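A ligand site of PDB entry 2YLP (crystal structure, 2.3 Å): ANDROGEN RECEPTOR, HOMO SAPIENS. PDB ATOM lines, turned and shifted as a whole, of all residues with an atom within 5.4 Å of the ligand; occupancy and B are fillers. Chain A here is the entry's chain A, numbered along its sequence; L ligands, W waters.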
ATOM      1  N   LEU A  38      24.175  13.164  31.012  1.00  0.00           N
ATOM      2  CA  LEU A  38      23.327  14.038  31.819  1.00  0.00           C
ATOM      3  C   LEU A  38      24.068  15.191  32.523  1.00  0.00           C
ATOM      4  O   LEU A  38      23.523  16.319  32.568  1.00  0.00           O
ATOM      5  CB  LEU A  38      22.476  13.258  32.802  1.00  0.00           C
ATOM      6  CG  LEU A  38      21.127  12.824  32.247  1.00  0.00           C
ATOM      7  CD1 LEU A  38      20.217  14.035  31.993  1.00  0.00           C
ATOM      8  CD2 LEU A  38      21.281  11.959  30.998  1.00  0.00           C
ATOM      9  N   LEU A  41      24.547  17.787  29.924  1.00  0.00           N
ATOM     10  CA  LEU A  41      23.252  18.435  29.559  1.00  0.00           C
ATOM     11  C   LEU A  41      22.950  19.478  30.627  1.00  0.00           C
ATOM     12  O   LEU A  41      22.541  20.583  30.295  1.00  0.00           O
ATOM     13  CB  LEU A  41      22.107  17.416  29.441  1.00  0.00           C
ATOM     14  CG  LEU A  41      21.932  16.729  28.060  1.00  0.00           C
ATOM     15  CD1 LEU A  41      20.775  15.773  28.154  1.00  0.00           C
ATOM     16  CD2 LEU A  41      21.691  17.690  26.906  1.00  0.00           C
ATOM     17  N   ASN A  42      23.165  19.087  31.897  1.00  0.00           N
ATOM     18  CA  ASN A  42      23.126  19.990  33.082  1.00  0.00           C
ATOM     19  C   ASN A  42      24.086  21.198  32.996  1.00  0.00           C
ATOM     20  O   ASN A  42      23.724  22.307  33.337  1.00  0.00           O
ATOM     21  CB  ASN A  42      23.377  19.223  34.407  1.00  0.00           C
ATOM     22  CG  ASN A  42      22.215  18.303  34.778  1.00  0.00           C
ATOM     23  OD1 ASN A  42      21.092  18.421  34.246  1.00  0.00           O
ATOM     24  ND2 ASN A  42      22.466  17.394  35.730  1.00  0.00           N
ATOM     25  N   LEU A  44      25.338  22.401  30.174  1.00  0.00           N
ATOM     26  CA  LEU A  44      24.753  23.097  29.052  1.00  0.00           C
ATOM     27  C   LEU A  44      23.589  23.928  29.564  1.00  0.00           C
ATOM     28  O   LEU A  44      23.450  25.062  29.156  1.00  0.00           O
ATOM     29  CB  LEU A  44      24.252  22.096  27.972  1.00  0.00           C
ATOM     30  CG  LEU A  44      23.670  22.882  26.779  1.00  0.00           C
ATOM     31  CD1 LEU A  44      24.779  23.846  26.209  1.00  0.00           C
ATOM     32  CD2 LEU A  44      23.103  21.947  25.679  1.00  0.00           C
ATOM     33  N   GLY A  45      22.747  23.370  30.438  1.00  0.00           N
ATOM     34  CA  GLY A  45      21.612  24.151  30.935  1.00  0.00           C
ATOM     35  C   GLY A  45      22.066  25.386  31.686  1.00  0.00           C
ATOM     36  O   GLY A  45      21.561  26.487  31.462  1.00  0.00           O
ATOM     37  N   GLN A  48      23.309  27.877  29.114  1.00  0.00           N
ATOM     38  CA  GLN A  48      22.197  28.528  28.394  1.00  0.00           C
ATOM     39  C   GLN A  48      21.414  29.533  29.256  1.00  0.00           C
ATOM     40  O   GLN A  48      20.951  30.535  28.748  1.00  0.00           O
ATOM     41  CB  GLN A  48      21.328  27.545  27.665  1.00  0.00           C
ATOM     42  CG  GLN A  48      22.047  26.776  26.607  1.00  0.00           C
ATOM     43  CD  GLN A  48      21.067  26.100  25.632  1.00  0.00           C
ATOM     44  OE1 GLN A  48      19.841  26.310  25.717  1.00  0.00           O
ATOM     45  NE2 GLN A  48      21.580  25.306  24.715  1.00  0.00           N
ATOM     46  N   TRP A  78      12.328  28.728  31.315  1.00  0.00           N
ATOM     47  CA  TRP A  78      13.574  28.360  30.618  1.00  0.00           C
ATOM     48  C   TRP A  78      13.543  27.024  29.906  1.00  0.00           C
ATOM     49  O   TRP A  78      14.133  26.871  28.793  1.00  0.00           O
ATOM     50  CB  TRP A  78      14.765  28.362  31.562  1.00  0.00           C
ATOM     51  CG  TRP A  78      14.560  27.526  32.757  1.00  0.00           C
ATOM     52  CD1 TRP A  78      13.897  27.885  33.886  1.00  0.00           C
ATOM     53  CD2 TRP A  78      15.047  26.182  32.983  1.00  0.00           C
ATOM     54  NE1 TRP A  78      13.928  26.851  34.807  1.00  0.00           N
ATOM     55  CE2 TRP A  78      14.609  25.793  34.279  1.00  0.00           C
ATOM     56  CE3 TRP A  78      15.790  25.265  32.207  1.00  0.00           C
ATOM     57  CZ2 TRP A  78      14.886  24.505  34.833  1.00  0.00           C
ATOM     58  CZ3 TRP A  78      16.087  24.003  32.739  1.00  0.00           C
ATOM     59  CH2 TRP A  78      15.639  23.624  34.055  1.00  0.00           C
ATOM     60  N   MET A  79      12.941  26.017  30.555  1.00  0.00           N
ATOM     61  CA  MET A  79      12.910  24.676  29.964  1.00  0.00           C
ATOM     62  C   MET A  79      12.230  24.736  28.588  1.00  0.00           C
ATOM     63  O   MET A  79      12.754  24.221  27.616  1.00  0.00           O
ATOM     64  CB  MET A  79      12.160  23.636  30.837  1.00  0.00           C
ATOM     65  CG  MET A  79      12.131  22.252  30.197  1.00  0.00           C
ATOM     66  SD  MET A  79      13.758  21.475  30.353  1.00  0.00           S
ATOM     67  CE  MET A  79      13.669  21.068  32.122  1.00  0.00           C
ATOM     68  N   MET A  82      14.409  26.762  25.916  1.00  0.00           N
ATOM     69  CA  MET A  82      15.552  25.958  25.509  1.00  0.00           C
ATOM     70  C   MET A  82      15.160  24.743  24.675  1.00  0.00           C
ATOM     71  O   MET A  82      15.825  24.427  23.710  1.00  0.00           O
ATOM     72  CB  MET A  82      16.357  25.506  26.749  1.00  0.00           C
ATOM     73  CG  MET A  82      17.063  26.664  27.443  1.00  0.00           C
ATOM     74  SD  MET A  82      17.916  26.157  28.955  1.00  0.00           S
ATOM     75  CE  MET A  82      18.331  27.774  29.638  1.00  0.00           C
ATOM     76  N   VAL A  83      14.091  24.054  25.048  1.00  0.00           N
ATOM     77  CA  VAL A  83      13.621  22.952  24.223  1.00  0.00           C
ATOM     78  C   VAL A  83      13.260  23.478  22.832  1.00  0.00           C
ATOM     79  O   VAL A  83      13.649  22.876  21.829  1.00  0.00           O
ATOM     80  CB  VAL A  83      12.425  22.242  24.854  1.00  0.00           C
ATOM     81  CG1 VAL A  83      11.828  21.229  23.924  1.00  0.00           C
ATOM     82  CG2 VAL A  83      12.906  21.561  26.115  1.00  0.00           C
ATOM     83  N   MET A  86      16.424  24.488  20.795  1.00  0.00           N
ATOM     84  CA  MET A  86      17.196  23.289  20.476  1.00  0.00           C
ATOM     85  C   MET A  86      16.526  22.587  19.267  1.00  0.00           C
ATOM     86  O   MET A  86      17.207  22.197  18.340  1.00  0.00           O
ATOM     87  CB  MET A  86      17.291  22.375  21.694  1.00  0.00           C
ATOM     88  CG  MET A  86      18.131  21.135  21.482  1.00  0.00           C
ATOM     89  SD  MET A  86      17.237  19.795  20.646  1.00  0.00           S
ATOM     90  CE  MET A  86      16.402  19.112  22.090  1.00  0.00           C
ATOM     91  N   ARG A  89      17.499  24.620  16.271  1.00  0.00           N
ATOM     92  CA  ARG A  89      18.881  24.239  15.924  1.00  0.00           C
ATOM     93  C   ARG A  89      18.910  22.878  15.219  1.00  0.00           C
ATOM     94  O   ARG A  89      19.504  22.726  14.167  1.00  0.00           O
ATOM     95  CB  ARG A  89      19.776  24.112  17.166  1.00  0.00           C
ATOM     96  CG  ARG A  89      20.238  25.450  17.775  1.00  0.00           C
ATOM     97  CD  ARG A  89      21.349  25.239  18.808  1.00  0.00           C
ATOM     98  NE  ARG A  89      20.952  24.356  19.911  1.00  0.00           N
ATOM     99  CZ  ARG A  89      20.286  24.740  21.011  1.00  0.00           C
ATOM    100  NH1 ARG A  89      19.941  26.022  21.192  1.00  0.00           N
ATOM    101  NH2 ARG A  89      19.960  23.842  21.924  1.00  0.00           N
ATOM    102  N   PHE A 101      21.653  19.488  20.800  1.00  0.00           N
ATOM    103  CA  PHE A 101      21.836  20.255  22.029  1.00  0.00           C
ATOM    104  C   PHE A 101      22.911  21.317  21.895  1.00  0.00           C
ATOM    105  O   PHE A 101      22.681  22.437  22.281  1.00  0.00           O
ATOM    106  CB  PHE A 101      22.091  19.328  23.218  1.00  0.00           C
ATOM    107  CG  PHE A 101      20.926  18.468  23.515  1.00  0.00           C
ATOM    108  CD1 PHE A 101      19.850  18.955  24.261  1.00  0.00           C
ATOM    109  CD2 PHE A 101      20.849  17.195  23.018  1.00  0.00           C
ATOM    110  CE1 PHE A 101      18.738  18.143  24.518  1.00  0.00           C
ATOM    111  CE2 PHE A 101      19.717  16.347  23.286  1.00  0.00           C
ATOM    112  CZ  PHE A 101      18.664  16.836  24.038  1.00  0.00           C
ATOM    113  N   MET A 117      16.375   8.887  28.433  1.00  0.00           N
ATOM    114  CA  MET A 117      15.304   9.828  28.121  1.00  0.00           C
ATOM    115  C   MET A 117      14.819   9.561  26.751  1.00  0.00           C
ATOM    116  O   MET A 117      14.453  10.501  26.024  1.00  0.00           O
ATOM    117  CB  MET A 117      15.832  11.251  28.051  1.00  0.00           C
ATOM    118  CG  MET A 117      16.414  11.819  29.290  1.00  0.00           C
ATOM    119  SD  MET A 117      16.483  13.601  28.983  1.00  0.00           S
ATOM    120  CE  MET A 117      18.076  13.722  28.216  1.00  0.00           C
ATOM    121  N   MET A 124      10.857  15.405  21.508  1.00  0.00           N
ATOM    122  CA  MET A 124      11.614  16.597  21.082  1.00  0.00           C
ATOM    123  C   MET A 124      11.931  16.514  19.594  1.00  0.00           C
ATOM    124  O   MET A 124      11.809  17.523  18.887  1.00  0.00           O
ATOM    125  CB  MET A 124      12.915  16.778  21.889  1.00  0.00           C
ATOM    126  CG  MET A 124      12.651  17.178  23.334  1.00  0.00           C
ATOM    127  SD  MET A 124      14.112  17.572  24.368  1.00  0.00           S
ATOM    128  CE  MET A 124      14.573  15.966  25.002  1.00  0.00           C
ATOM    129  N   LEU A 210      10.050  16.980  31.047  1.00  0.00           N
ATOM    130  CA  LEU A 210      11.453  17.216  31.375  1.00  0.00           C
ATOM    131  C   LEU A 210      11.635  17.839  32.760  1.00  0.00           C
ATOM    132  O   LEU A 210      12.662  17.620  33.429  1.00  0.00           O
ATOM    133  CB  LEU A 210      12.143  18.033  30.285  1.00  0.00           C
ATOM    134  CG  LEU A 210      12.228  17.283  28.944  1.00  0.00           C
ATOM    135  CD1 LEU A 210      12.414  18.310  27.853  1.00  0.00           C
ATOM    136  CD2 LEU A 210      13.354  16.253  28.945  1.00  0.00           C
ATOM    137  N   PHE A 213      11.355  14.676  34.951  1.00  0.00           N
ATOM    138  CA  PHE A 213      12.600  13.981  34.810  1.00  0.00           C
ATOM    139  C   PHE A 213      13.752  14.599  35.621  1.00  0.00           C
ATOM    140  O   PHE A 213      14.379  13.928  36.427  1.00  0.00           O
ATOM    141  CB  PHE A 213      12.978  13.830  33.335  1.00  0.00           C
ATOM    142  CG  PHE A 213      14.099  12.870  33.103  1.00  0.00           C
ATOM    143  CD1 PHE A 213      15.433  13.256  33.347  1.00  0.00           C
ATOM    144  CD2 PHE A 213      13.846  11.566  32.696  1.00  0.00           C
ATOM    145  CE1 PHE A 213      16.487  12.362  33.150  1.00  0.00           C
ATOM    146  CE2 PHE A 213      14.899  10.671  32.499  1.00  0.00           C
ATOM    147  CZ  PHE A 213      16.214  11.068  32.718  1.00  0.00           C
ATOM    148  N   THR A 214      14.029  15.881  35.364  1.00  0.00           N
ATOM    149  CA  THR A 214      15.186  16.509  35.972  1.00  0.00           C
ATOM    150  C   THR A 214      14.968  16.633  37.474  1.00  0.00           C
ATOM    151  O   THR A 214      15.926  16.585  38.267  1.00  0.00           O
ATOM    152  CB  THR A 214      15.549  17.903  35.345  1.00  0.00           C
ATOM    153  OG1 THR A 214      16.828  18.296  35.820  1.00  0.00           O
ATOM    154  CG2 THR A 214      14.565  19.039  35.736  1.00  0.00           C
ATOM    155  N   LEU A 217      15.745  13.312  38.989  1.00  0.00           N
ATOM    156  CA  LEU A 217      17.142  13.044  38.848  1.00  0.00           C
ATOM    157  C   LEU A 217      17.905  13.908  39.845  1.00  0.00           C
ATOM    158  O   LEU A 217      18.878  13.434  40.429  1.00  0.00           O
ATOM    159  CB  LEU A 217      17.577  13.322  37.414  1.00  0.00           C
ATOM    160  CG  LEU A 217      19.063  13.240  37.087  1.00  0.00           C
ATOM    161  CD1 LEU A 217      19.580  11.788  37.358  1.00  0.00           C
ATOM    162  CD2 LEU A 217      19.244  13.656  35.636  1.00  0.00           C
ATOM    163  N   PHE A 228      24.850  18.495  39.133  1.00  0.00           N
ATOM    164  CA  PHE A 228      24.038  19.671  38.854  1.00  0.00           C
ATOM    165  C   PHE A 228      24.858  20.856  39.341  1.00  0.00           C
ATOM    166  O   PHE A 228      25.307  20.880  40.490  1.00  0.00           O
ATOM    167  CB  PHE A 228      22.721  19.602  39.616  1.00  0.00           C
ATOM    168  CG  PHE A 228      21.724  18.619  39.023  1.00  0.00           C
ATOM    169  CD1 PHE A 228      21.893  17.254  39.178  1.00  0.00           C
ATOM    170  CD2 PHE A 228      20.624  19.085  38.310  1.00  0.00           C
ATOM    171  CE1 PHE A 228      20.956  16.349  38.627  1.00  0.00           C
ATOM    172  CE2 PHE A 228      19.654  18.160  37.776  1.00  0.00           C
ATOM    173  CZ  PHE A 228      19.832  16.823  37.919  1.00  0.00           C
ATOM    174  N   MET A 232      21.236  25.485  38.464  1.00  0.00           N
ATOM    175  CA  MET A 232      20.263  24.506  38.008  1.00  0.00           C
ATOM    176  C   MET A 232      19.733  23.762  39.228  1.00  0.00           C
ATOM    177  O   MET A 232      18.538  23.498  39.336  1.00  0.00           O
ATOM    178  CB  MET A 232      20.886  23.538  36.985  1.00  0.00           C
ATOM    179  CG  MET A 232      21.257  24.140  35.645  1.00  0.00           C
ATOM    180  SD  MET A 232      19.864  24.303  34.490  1.00  0.00           S
ATOM    181  CE  MET A 232      19.658  22.610  33.986  1.00  0.00           C
ATOM    182  N   ILE A 236      15.978  23.985  40.220  1.00  0.00           N
ATOM    183  CA  ILE A 236      15.206  22.734  40.139  1.00  0.00           C
ATOM    184  C   ILE A 236      14.675  22.314  41.493  1.00  0.00           C
ATOM    185  O   ILE A 236      13.711  21.571  41.533  1.00  0.00           O
ATOM    186  CB  ILE A 236      15.980  21.631  39.406  1.00  0.00           C
ATOM    187  CG1 ILE A 236      16.128  22.041  37.917  1.00  0.00           C
ATOM    188  CG2 ILE A 236      15.332  20.274  39.568  1.00  0.00           C
ATOM    189  CD1 ILE A 236      17.243  21.274  37.197  1.00  0.00           C
HETATM  190  C1  LIG L   1      19.801  21.962  27.947  1.00  0.00           C
HETATM  191  C2  LIG L   1      19.833  22.985  26.815  1.00  0.00           C
HETATM  192  C3  LIG L   1      19.046  22.460  25.638  1.00  0.00           C
HETATM  193  O1  LIG L   1      19.307  22.850  24.505  1.00  0.00           O
HETATM  194  C4  LIG L   1      17.949  21.490  25.882  1.00  0.00           C
HETATM  195  C5  LIG L   1      17.633  20.980  27.093  1.00  0.00           C
HETATM  196  C6  LIG L   1      16.472  19.966  27.187  1.00  0.00           C
HETATM  197  C7  LIG L   1      16.759  18.864  28.231  1.00  0.00           C
HETATM  198  C8  LIG L   1      17.364  19.397  29.522  1.00  0.00           C
HETATM  199  C9  LIG L   1      18.645  20.247  29.287  1.00  0.00           C
HETATM  200  C10 LIG L   1      18.410  21.427  28.331  1.00  0.00           C
HETATM  201  C11 LIG L   1      19.333  20.770  30.589  1.00  0.00           C
HETATM  202  C12 LIG L   1      19.524  19.662  31.663  1.00  0.00           C
HETATM  203  C13 LIG L   1      18.269  18.799  31.852  1.00  0.00           C
HETATM  204  C14 LIG L   1      17.721  18.297  30.507  1.00  0.00           C
HETATM  205  C15 LIG L   1      16.678  17.238  30.878  1.00  0.00           C
HETATM  206  C16 LIG L   1      17.349  16.507  32.039  1.00  0.00           C
HETATM  207  C17 LIG L   1      18.477  17.431  32.518  1.00  0.00           C
HETATM  208  O2  LIG L   1      18.504  17.441  33.948  1.00  0.00           O
HETATM  209  C18 LIG L   1      17.184  19.671  32.543  1.00  0.00           C
HETATM  210  C19 LIG L   1      17.640  22.513  29.103  1.00  0.00           C
HETATM  211  O   HOH W   1      18.535  25.639  23.615  1.00  0.00           O
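An oxygen (O2) of the ligand is in hydrogen-bond range of the side-chain hydroxyl (OG1) of Thr 214, at 2.7 Å. An oxygen (O2) of the ligand sits at hydrogen-bond distance from the side-chain amide oxygen (OD1) of Asn 42 (2.8 Å). O1 of the ligand is in hydrogen-bond range of NH2 of Arg 89, 2.8 Å away. The side-chain amide nitrogen (NE2) of Gln 48 sits at hydrogen-bond distance from an oxygen (O1) of the ligand, at 3.4 Å.
The backbone carbonyl oxygen of Phe 101 is in hydrogen-bond range of the guanidinium group of Arg 89, 3.1 Å away. OE1 of Gln 48 lies close to SD of Met 82, 3.8 Å away.
Residues that only touch the ligand: Leu 38 (3.8 Å), Leu 41 (3.2 Å), Leu 44 (3.6 Å), Met 79 (3.8 Å), Met 82 (3.7 Å), Met 86 (3.5 Å), Phe 101 (3.6 Å), Leu 210 (3.97 Å), Phe 213 (3.99 Å) and Met 232 (3.8 Å). Of the 22 residues printed, 14 come within 4 Å of the ligand. Along chain A the residues within 4 Å of the ligand span positions 38 to 232.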
